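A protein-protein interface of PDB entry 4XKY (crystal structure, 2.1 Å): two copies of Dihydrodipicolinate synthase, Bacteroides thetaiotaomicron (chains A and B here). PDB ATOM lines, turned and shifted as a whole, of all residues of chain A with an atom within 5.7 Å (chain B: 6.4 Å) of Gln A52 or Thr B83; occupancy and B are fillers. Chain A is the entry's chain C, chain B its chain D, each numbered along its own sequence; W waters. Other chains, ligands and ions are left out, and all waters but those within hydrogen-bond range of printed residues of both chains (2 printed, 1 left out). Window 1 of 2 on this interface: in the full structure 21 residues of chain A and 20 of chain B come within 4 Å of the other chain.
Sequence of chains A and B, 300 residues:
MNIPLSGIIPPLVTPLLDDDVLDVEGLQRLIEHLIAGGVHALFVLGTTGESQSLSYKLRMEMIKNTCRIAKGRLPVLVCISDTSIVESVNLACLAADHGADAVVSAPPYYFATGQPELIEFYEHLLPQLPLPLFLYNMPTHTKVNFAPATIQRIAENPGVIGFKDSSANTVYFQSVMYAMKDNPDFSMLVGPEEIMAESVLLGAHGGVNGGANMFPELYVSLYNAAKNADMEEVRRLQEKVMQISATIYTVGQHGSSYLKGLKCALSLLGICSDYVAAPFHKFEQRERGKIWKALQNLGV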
ATOM      1  N   THR A  47      -3.910  -5.577 -20.332  1.00  0.00           N
ATOM      2  CA  THR A  47      -2.575  -5.383 -20.910  1.00  0.00           C
ATOM      3  C   THR A  47      -2.673  -5.069 -22.399  1.00  0.00           C
ATOM      4  O   THR A  47      -2.018  -4.154 -22.910  1.00  0.00           O
ATOM      5  CB  THR A  47      -1.736  -6.675 -20.761  1.00  0.00           C
ATOM      6  OG1 THR A  47      -1.722  -7.081 -19.388  1.00  0.00           O
ATOM      7  CG2 THR A  47      -0.292  -6.467 -21.230  1.00  0.00           C
ATOM      8  N   GLU A  50      -3.225  -1.459 -23.093  1.00  0.00           N
ATOM      9  CA  GLU A  50      -2.198  -0.445 -22.722  1.00  0.00           C
ATOM     10  C   GLU A  50      -2.561   0.364 -21.478  1.00  0.00           C
ATOM     11  O   GLU A  50      -2.150   1.528 -21.336  1.00  0.00           O
ATOM     12  CB  GLU A  50      -1.936   0.558 -23.869  1.00  0.00           C
ATOM     13  CG  GLU A  50      -1.168   0.001 -25.054  1.00  0.00           C
ATOM     14  CD  GLU A  50      -1.209   0.918 -26.277  1.00  0.00           C
ATOM     15  OE1 GLU A  50      -2.111   0.730 -27.115  1.00  0.00           O
ATOM     16  OE2 GLU A  50      -0.348   1.823 -26.420  1.00  0.00           O
ATOM     17  N   SER A  51      -3.310  -0.235 -20.566  1.00  0.00           N
ATOM     18  CA  SER A  51      -3.937   0.560 -19.518  1.00  0.00           C
ATOM     19  C   SER A  51      -2.935   1.442 -18.781  1.00  0.00           C
ATOM     20  O   SER A  51      -3.110   2.641 -18.667  1.00  0.00           O
ATOM     21  CB  SER A  51      -4.627  -0.338 -18.507  1.00  0.00           C
ATOM     22  OG  SER A  51      -5.397   0.459 -17.629  1.00  0.00           O
ATOM     23  N   GLN A  52      -1.881   0.820 -18.291  1.00  0.00           N
ATOM     24  CA  GLN A  52      -0.893   1.489 -17.440  1.00  0.00           C
ATOM     25  C   GLN A  52      -0.176   2.663 -18.108  1.00  0.00           C
ATOM     26  O   GLN A  52       0.221   3.620 -17.437  1.00  0.00           O
ATOM     27  CB  GLN A  52       0.147   0.470 -17.001  1.00  0.00           C
ATOM     28  CG  GLN A  52       0.937  -0.144 -18.154  1.00  0.00           C
ATOM     29  CD  GLN A  52       1.821  -1.284 -17.696  1.00  0.00           C
ATOM     30  OE1 GLN A  52       2.619  -1.126 -16.771  1.00  0.00           O
ATOM     31  NE2 GLN A  52       1.688  -2.439 -18.336  1.00  0.00           N
ATOM     32  N   SER A  53       0.006   2.555 -19.427  1.00  0.00           N
ATOM     33  CA  SER A  53       0.631   3.594 -20.249  1.00  0.00           C
ATOM     34  C   SER A  53      -0.254   4.786 -20.513  1.00  0.00           C
ATOM     35  O   SER A  53       0.238   5.820 -20.939  1.00  0.00           O
ATOM     36  CB  SER A  53       1.008   3.017 -21.604  1.00  0.00           C
ATOM     37  OG  SER A  53       2.034   2.083 -21.426  1.00  0.00           O
ATOM     38  N   LEU A  54      -1.557   4.640 -20.312  1.00  0.00           N
ATOM     39  CA  LEU A  54      -2.472   5.738 -20.587  1.00  0.00           C
ATOM     40  C   LEU A  54      -2.716   6.595 -19.363  1.00  0.00           C
ATOM     41  O   LEU A  54      -2.662   6.117 -18.238  1.00  0.00           O
ATOM     42  CB  LEU A  54      -3.805   5.214 -21.105  1.00  0.00           C
ATOM     43  CG  LEU A  54      -3.732   4.238 -22.280  1.00  0.00           C
ATOM     44  CD1 LEU A  54      -5.125   3.780 -22.635  1.00  0.00           C
ATOM     45  CD2 LEU A  54      -3.038   4.835 -23.492  1.00  0.00           C
ATOM     46  N   ARG A  59      -8.213   6.571 -19.606  1.00  0.00           N
ATOM     47  CA  ARG A  59      -8.756   5.318 -19.128  1.00  0.00           C
ATOM     48  C   ARG A  59     -10.240   5.487 -18.803  1.00  0.00           C
ATOM     49  O   ARG A  59     -11.056   4.602 -19.075  1.00  0.00           O
ATOM     50  CB  ARG A  59      -7.972   4.837 -17.918  1.00  0.00           C
ATOM     51  CG  ARG A  59      -6.580   4.374 -18.304  1.00  0.00           C
ATOM     52  CD  ARG A  59      -6.016   3.391 -17.303  1.00  0.00           C
ATOM     53  NE  ARG A  59      -5.282   4.052 -16.249  1.00  0.00           N
ATOM     54  CZ  ARG A  59      -4.962   3.488 -15.090  1.00  0.00           C
ATOM     55  NH1 ARG A  59      -5.305   2.220 -14.818  1.00  0.00           N
ATOM     56  NH2 ARG A  59      -4.296   4.211 -14.199  1.00  0.00           N
ATOM     57  N   THR A  83      -1.379   0.786  -9.986  1.00  0.00           N
ATOM     58  CA  THR A  83      -0.405   0.864  -8.907  1.00  0.00           C
ATOM     59  C   THR A  83      -1.008   1.509  -7.656  1.00  0.00           C
ATOM     60  O   THR A  83      -0.546   1.242  -6.562  1.00  0.00           O
ATOM     61  CB  THR A  83       0.876   1.644  -9.315  1.00  0.00           C
ATOM     62  OG1 THR A  83       0.531   2.967  -9.735  1.00  0.00           O
ATOM     63  CG2 THR A  83       1.611   0.920 -10.435  1.00  0.00           C
ATOM     64  N   TYR A 109       2.228  -4.457  -9.653  1.00  0.00           N
ATOM     65  CA  TYR A 109       3.520  -5.081 -10.060  1.00  0.00           C
ATOM     66  C   TYR A 109       4.573  -5.143  -8.935  1.00  0.00           C
ATOM     67  O   TYR A 109       5.261  -6.146  -8.777  1.00  0.00           O
ATOM     68  CB  TYR A 109       4.114  -4.396 -11.325  1.00  0.00           C
ATOM     69  CG  TYR A 109       4.883  -3.110 -11.073  1.00  0.00           C
ATOM     70  CD1 TYR A 109       6.259  -3.125 -10.792  1.00  0.00           C
ATOM     71  CD2 TYR A 109       4.232  -1.876 -11.103  1.00  0.00           C
ATOM     72  CE1 TYR A 109       6.957  -1.941 -10.551  1.00  0.00           C
ATOM     73  CE2 TYR A 109       4.915  -0.692 -10.869  1.00  0.00           C
ATOM     74  CZ  TYR A 109       6.272  -0.724 -10.593  1.00  0.00           C
ATOM     75  OH  TYR A 109       6.922   0.467 -10.363  1.00  0.00           O
ATOM     76  N   ALA A 278       3.004   6.439 -26.410  1.00  0.00           N
ATOM     77  CA  ALA A 278       4.363   6.641 -25.892  1.00  0.00           C
ATOM     78  C   ALA A 278       4.442   6.014 -24.517  1.00  0.00           C
ATOM     79  O   ALA A 278       3.477   6.088 -23.769  1.00  0.00           O
ATOM     80  CB  ALA A 278       4.687   8.124 -25.794  1.00  0.00           C
ATOM     81  N   PRO A 279       5.604   5.445 -24.146  1.00  0.00           N
ATOM     82  CA  PRO A 279       6.935   5.511 -24.774  1.00  0.00           C
ATOM     83  C   PRO A 279       7.176   4.588 -26.003  1.00  0.00           C
ATOM     84  O   PRO A 279       8.251   4.641 -26.617  1.00  0.00           O
ATOM     85  CB  PRO A 279       7.846   5.076 -23.624  1.00  0.00           C
ATOM     86  CG  PRO A 279       7.014   4.050 -22.902  1.00  0.00           C
ATOM     87  CD  PRO A 279       5.624   4.631 -22.916  1.00  0.00           C
ATOM     88  N   ARG B  59      -0.105  12.601  -4.776  1.00  0.00           N
ATOM     89  CA  ARG B  59       1.232  12.892  -5.267  1.00  0.00           C
ATOM     90  C   ARG B  59       1.389  14.408  -5.457  1.00  0.00           C
ATOM     91  O   ARG B  59       2.400  14.998  -5.093  1.00  0.00           O
ATOM     92  CB  ARG B  59       1.504  12.147  -6.567  1.00  0.00           C
ATOM     93  CG  ARG B  59       1.667  10.640  -6.387  1.00  0.00           C
ATOM     94  CD  ARG B  59       2.526  10.024  -7.487  1.00  0.00           C
ATOM     95  NE  ARG B  59       1.734   9.448  -8.544  1.00  0.00           N
ATOM     96  CZ  ARG B  59       2.188   9.127  -9.745  1.00  0.00           C
ATOM     97  NH1 ARG B  59       3.474   9.304 -10.080  1.00  0.00           N
ATOM     98  NH2 ARG B  59       1.335   8.613 -10.615  1.00  0.00           N
ATOM     99  N   SER B  81       8.627  10.017 -12.156  1.00  0.00           N
ATOM    100  CA  SER B  81       8.435   8.699 -12.735  1.00  0.00           C
ATOM    101  C   SER B  81       6.982   8.261 -12.633  1.00  0.00           C
ATOM    102  O   SER B  81       6.330   8.428 -11.608  1.00  0.00           O
ATOM    103  CB  SER B  81       9.326   7.677 -12.034  1.00  0.00           C
ATOM    104  OG  SER B  81      10.682   8.056 -12.185  1.00  0.00           O
ATOM    105  N   ASP B  82       6.487   7.717 -13.726  1.00  0.00           N
ATOM    106  CA  ASP B  82       5.131   7.229 -13.774  1.00  0.00           C
ATOM    107  C   ASP B  82       5.017   6.264 -14.932  1.00  0.00           C
ATOM    108  O   ASP B  82       5.754   6.387 -15.886  1.00  0.00           O
ATOM    109  CB  ASP B  82       4.203   8.393 -14.024  1.00  0.00           C
ATOM    110  CG  ASP B  82       2.789   8.065 -13.710  1.00  0.00           C
ATOM    111  OD1 ASP B  82       2.412   8.261 -12.550  1.00  0.00           O
ATOM    112  OD2 ASP B  82       2.066   7.629 -14.621  1.00  0.00           O
ATOM    113  N   THR B  83       4.084   5.321 -14.849  1.00  0.00           N
ATOM    114  CA  THR B  83       3.774   4.458 -15.988  1.00  0.00           C
ATOM    115  C   THR B  83       3.224   5.240 -17.211  1.00  0.00           C
ATOM    116  O   THR B  83       3.415   4.800 -18.348  1.00  0.00           O
ATOM    117  CB  THR B  83       2.854   3.264 -15.567  1.00  0.00           C
ATOM    118  OG1 THR B  83       1.591   3.731 -15.059  1.00  0.00           O
ATOM    119  CG2 THR B  83       3.541   2.415 -14.484  1.00  0.00           C
ATOM    120  N   SER B  84       2.587   6.404 -16.972  1.00  0.00           N
ATOM    121  CA  SER B  84       2.090   7.300 -18.047  1.00  0.00           C
ATOM    122  C   SER B  84       2.961   8.552 -18.231  1.00  0.00           C
ATOM    123  O   SER B  84       3.075   9.370 -17.318  1.00  0.00           O
ATOM    124  CB  SER B  84       0.653   7.756 -17.737  1.00  0.00           C
ATOM    125  OG  SER B  84       0.282   8.941 -18.449  1.00  0.00           O
ATOM    126  N   ILE B  85       3.518   8.725 -19.422  1.00  0.00           N
ATOM    127  CA  ILE B  85       4.342   9.900 -19.738  1.00  0.00           C
ATOM    128  C   ILE B  85       3.535  11.195 -19.559  1.00  0.00           C
ATOM    129  O   ILE B  85       4.063  12.185 -19.075  1.00  0.00           O
ATOM    130  CB  ILE B  85       4.943   9.798 -21.160  1.00  0.00           C
ATOM    131  CG1 ILE B  85       5.733   8.500 -21.315  1.00  0.00           C
ATOM    132  CG2 ILE B  85       5.865  10.972 -21.494  1.00  0.00           C
ATOM    133  CD1 ILE B  85       6.587   8.122 -20.111  1.00  0.00           C
ATOM    134  N   PRO B 108       9.681   4.019 -17.503  1.00  0.00           N
ATOM    135  CA  PRO B 108       8.721   3.120 -16.829  1.00  0.00           C
ATOM    136  C   PRO B 108       9.145   1.634 -16.809  1.00  0.00           C
ATOM    137  O   PRO B 108       9.782   1.174 -17.746  1.00  0.00           O
ATOM    138  CB  PRO B 108       7.422   3.331 -17.617  1.00  0.00           C
ATOM    139  CG  PRO B 108       7.799   4.055 -18.871  1.00  0.00           C
ATOM    140  CD  PRO B 108       9.077   4.788 -18.602  1.00  0.00           C
ATOM    141  N   TYR B 109       8.777   0.907 -15.752  1.00  0.00           N
ATOM    142  CA  TYR B 109       9.302  -0.449 -15.498  1.00  0.00           C
ATOM    143  C   TYR B 109       9.232  -1.349 -16.737  1.00  0.00           C
ATOM    144  O   TYR B 109      10.228  -1.975 -17.124  1.00  0.00           O
ATOM    145  CB  TYR B 109       8.639  -1.112 -14.257  1.00  0.00           C
ATOM    146  CG  TYR B 109       7.182  -1.548 -14.388  1.00  0.00           C
ATOM    147  CD1 TYR B 109       6.841  -2.874 -14.696  1.00  0.00           C
ATOM    148  CD2 TYR B 109       6.143  -0.638 -14.174  1.00  0.00           C
ATOM    149  CE1 TYR B 109       5.512  -3.264 -14.811  1.00  0.00           C
ATOM    150  CE2 TYR B 109       4.813  -1.018 -14.282  1.00  0.00           C
ATOM    151  CZ  TYR B 109       4.495  -2.327 -14.601  1.00  0.00           C
ATOM    152  OH  TYR B 109       3.154  -2.673 -14.707  1.00  0.00           O
ATOM    153  N   TYR B 110       8.075  -1.339 -17.390  1.00  0.00           N
ATOM    154  CA  TYR B 110       7.796  -2.200 -18.548  1.00  0.00           C
ATOM    155  C   TYR B 110       8.538  -1.826 -19.843  1.00  0.00           C
ATOM    156  O   TYR B 110       8.287  -2.436 -20.882  1.00  0.00           O
ATOM    157  CB  TYR B 110       6.278  -2.206 -18.835  1.00  0.00           C
ATOM    158  CG  TYR B 110       5.707  -0.821 -19.120  1.00  0.00           C
ATOM    159  CD1 TYR B 110       5.706  -0.293 -20.409  1.00  0.00           C
ATOM    160  CD2 TYR B 110       5.193  -0.029 -18.087  1.00  0.00           C
ATOM    161  CE1 TYR B 110       5.204   0.979 -20.664  1.00  0.00           C
ATOM    162  CE2 TYR B 110       4.690   1.244 -18.330  1.00  0.00           C
ATOM    163  CZ  TYR B 110       4.695   1.743 -19.615  1.00  0.00           C
ATOM    164  OH  TYR B 110       4.203   3.002 -19.859  1.00  0.00           O
HETATM  165  O   HOH W   1       0.231   8.659 -20.932  1.00  0.00           O
HETATM  166  O   HOH W   2       0.276   4.097 -12.390  1.00  0.00           O
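The backbone carbonyl oxygen (O) of Gln A52 sits at hydrogen-bond distance from the side-chain hydroxyl (OG1) of Thr B83. The side-chain hydroxyl (OG) of Ser A53 lies within hydrogen-bond range of the side-chain hydroxyl (OH) of Tyr B110 (2.8 Å). OE1 of Gln A52 is in hydrogen-bond range of OH of Tyr B109.
Among the printed residues, merely in contact across the chains: Gln A52 with Ser B84 (3.7 Å), Gln A52 with Tyr B110 (3.1 Å), Ser A53 with Thr B83 (3.6 Å), Ser A53 with Ser B84 (3.7 Å), Leu A54 with Ser B84 (3.7 Å), Tyr A109 with Tyr B109 (3.3 Å) and Pro A279 with Tyr B110 (3.7 Å).
O of Thr B83 lies within hydrogen-bond range of OH of Tyr B110, at 2.5 Å. N of Ser B84 lies within hydrogen-bond range of OD2 of Asp B82.
Ser A51 touches none of the printed residues of chain B. Of chain B, only Thr B83 (2.7 Å), Ser B84 (3.7 Å), Tyr B109 (2.6 Å) and Tyr B110 (3.1 Å) come within 4 Å of Gln A52. Printed residues of chain B within 4 Å of Leu A54: Ser B84 (3.7 Å). Printed residues of chain B within 4 Å of Pro A279: Tyr B110. Thr B83 touches just these residues of chain A: Gln A52 (2.7 Å) and Ser A53 (3.6 Å). Of the printed residues of chain A, Ser B84 touches Gln A52 (3.7 Å), Ser A53 (3.7 Å) and Leu A54 (3.7 Å). Of the printed residues of chain A, Tyr B109 touches Gln A52 (2.6 Å) and Tyr A109 (3.3 Å). The nearest residue of chain B that does not touch Gln A52 is Asp B82 (5.2 Å).
Of the 9 printed residues of chain B, 4 touch a printed residue of chain A. Hydrophobic or aromatic side chains of chain A within 4 Å of the printed part of chain B: Tyr A109 and Pro A279. Among the printed residues, no Asp or Glu carboxylate lies within 4 Å of a Lys or Arg side-chain nitrogen of the other chain.
Tyr B109 touches its own counterpart, Tyr A109. Of the 10 pairs that touch across the chains among the printed residues, 1 has its exchanged pair printed and touching as well.
Water W1 lies within hydrogen-bond range of the side-chain hydroxyl of Ser B84 (2.5 Å) and the backbone carbonyl oxygen of Ser A53 (2.8 Å). Water W2 bridges the side-chain hydroxyl (OG1) of Thr A83 (2.9 Å) and the side-chain hydroxyl (OG1) of Thr B83 (3.0 Å).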
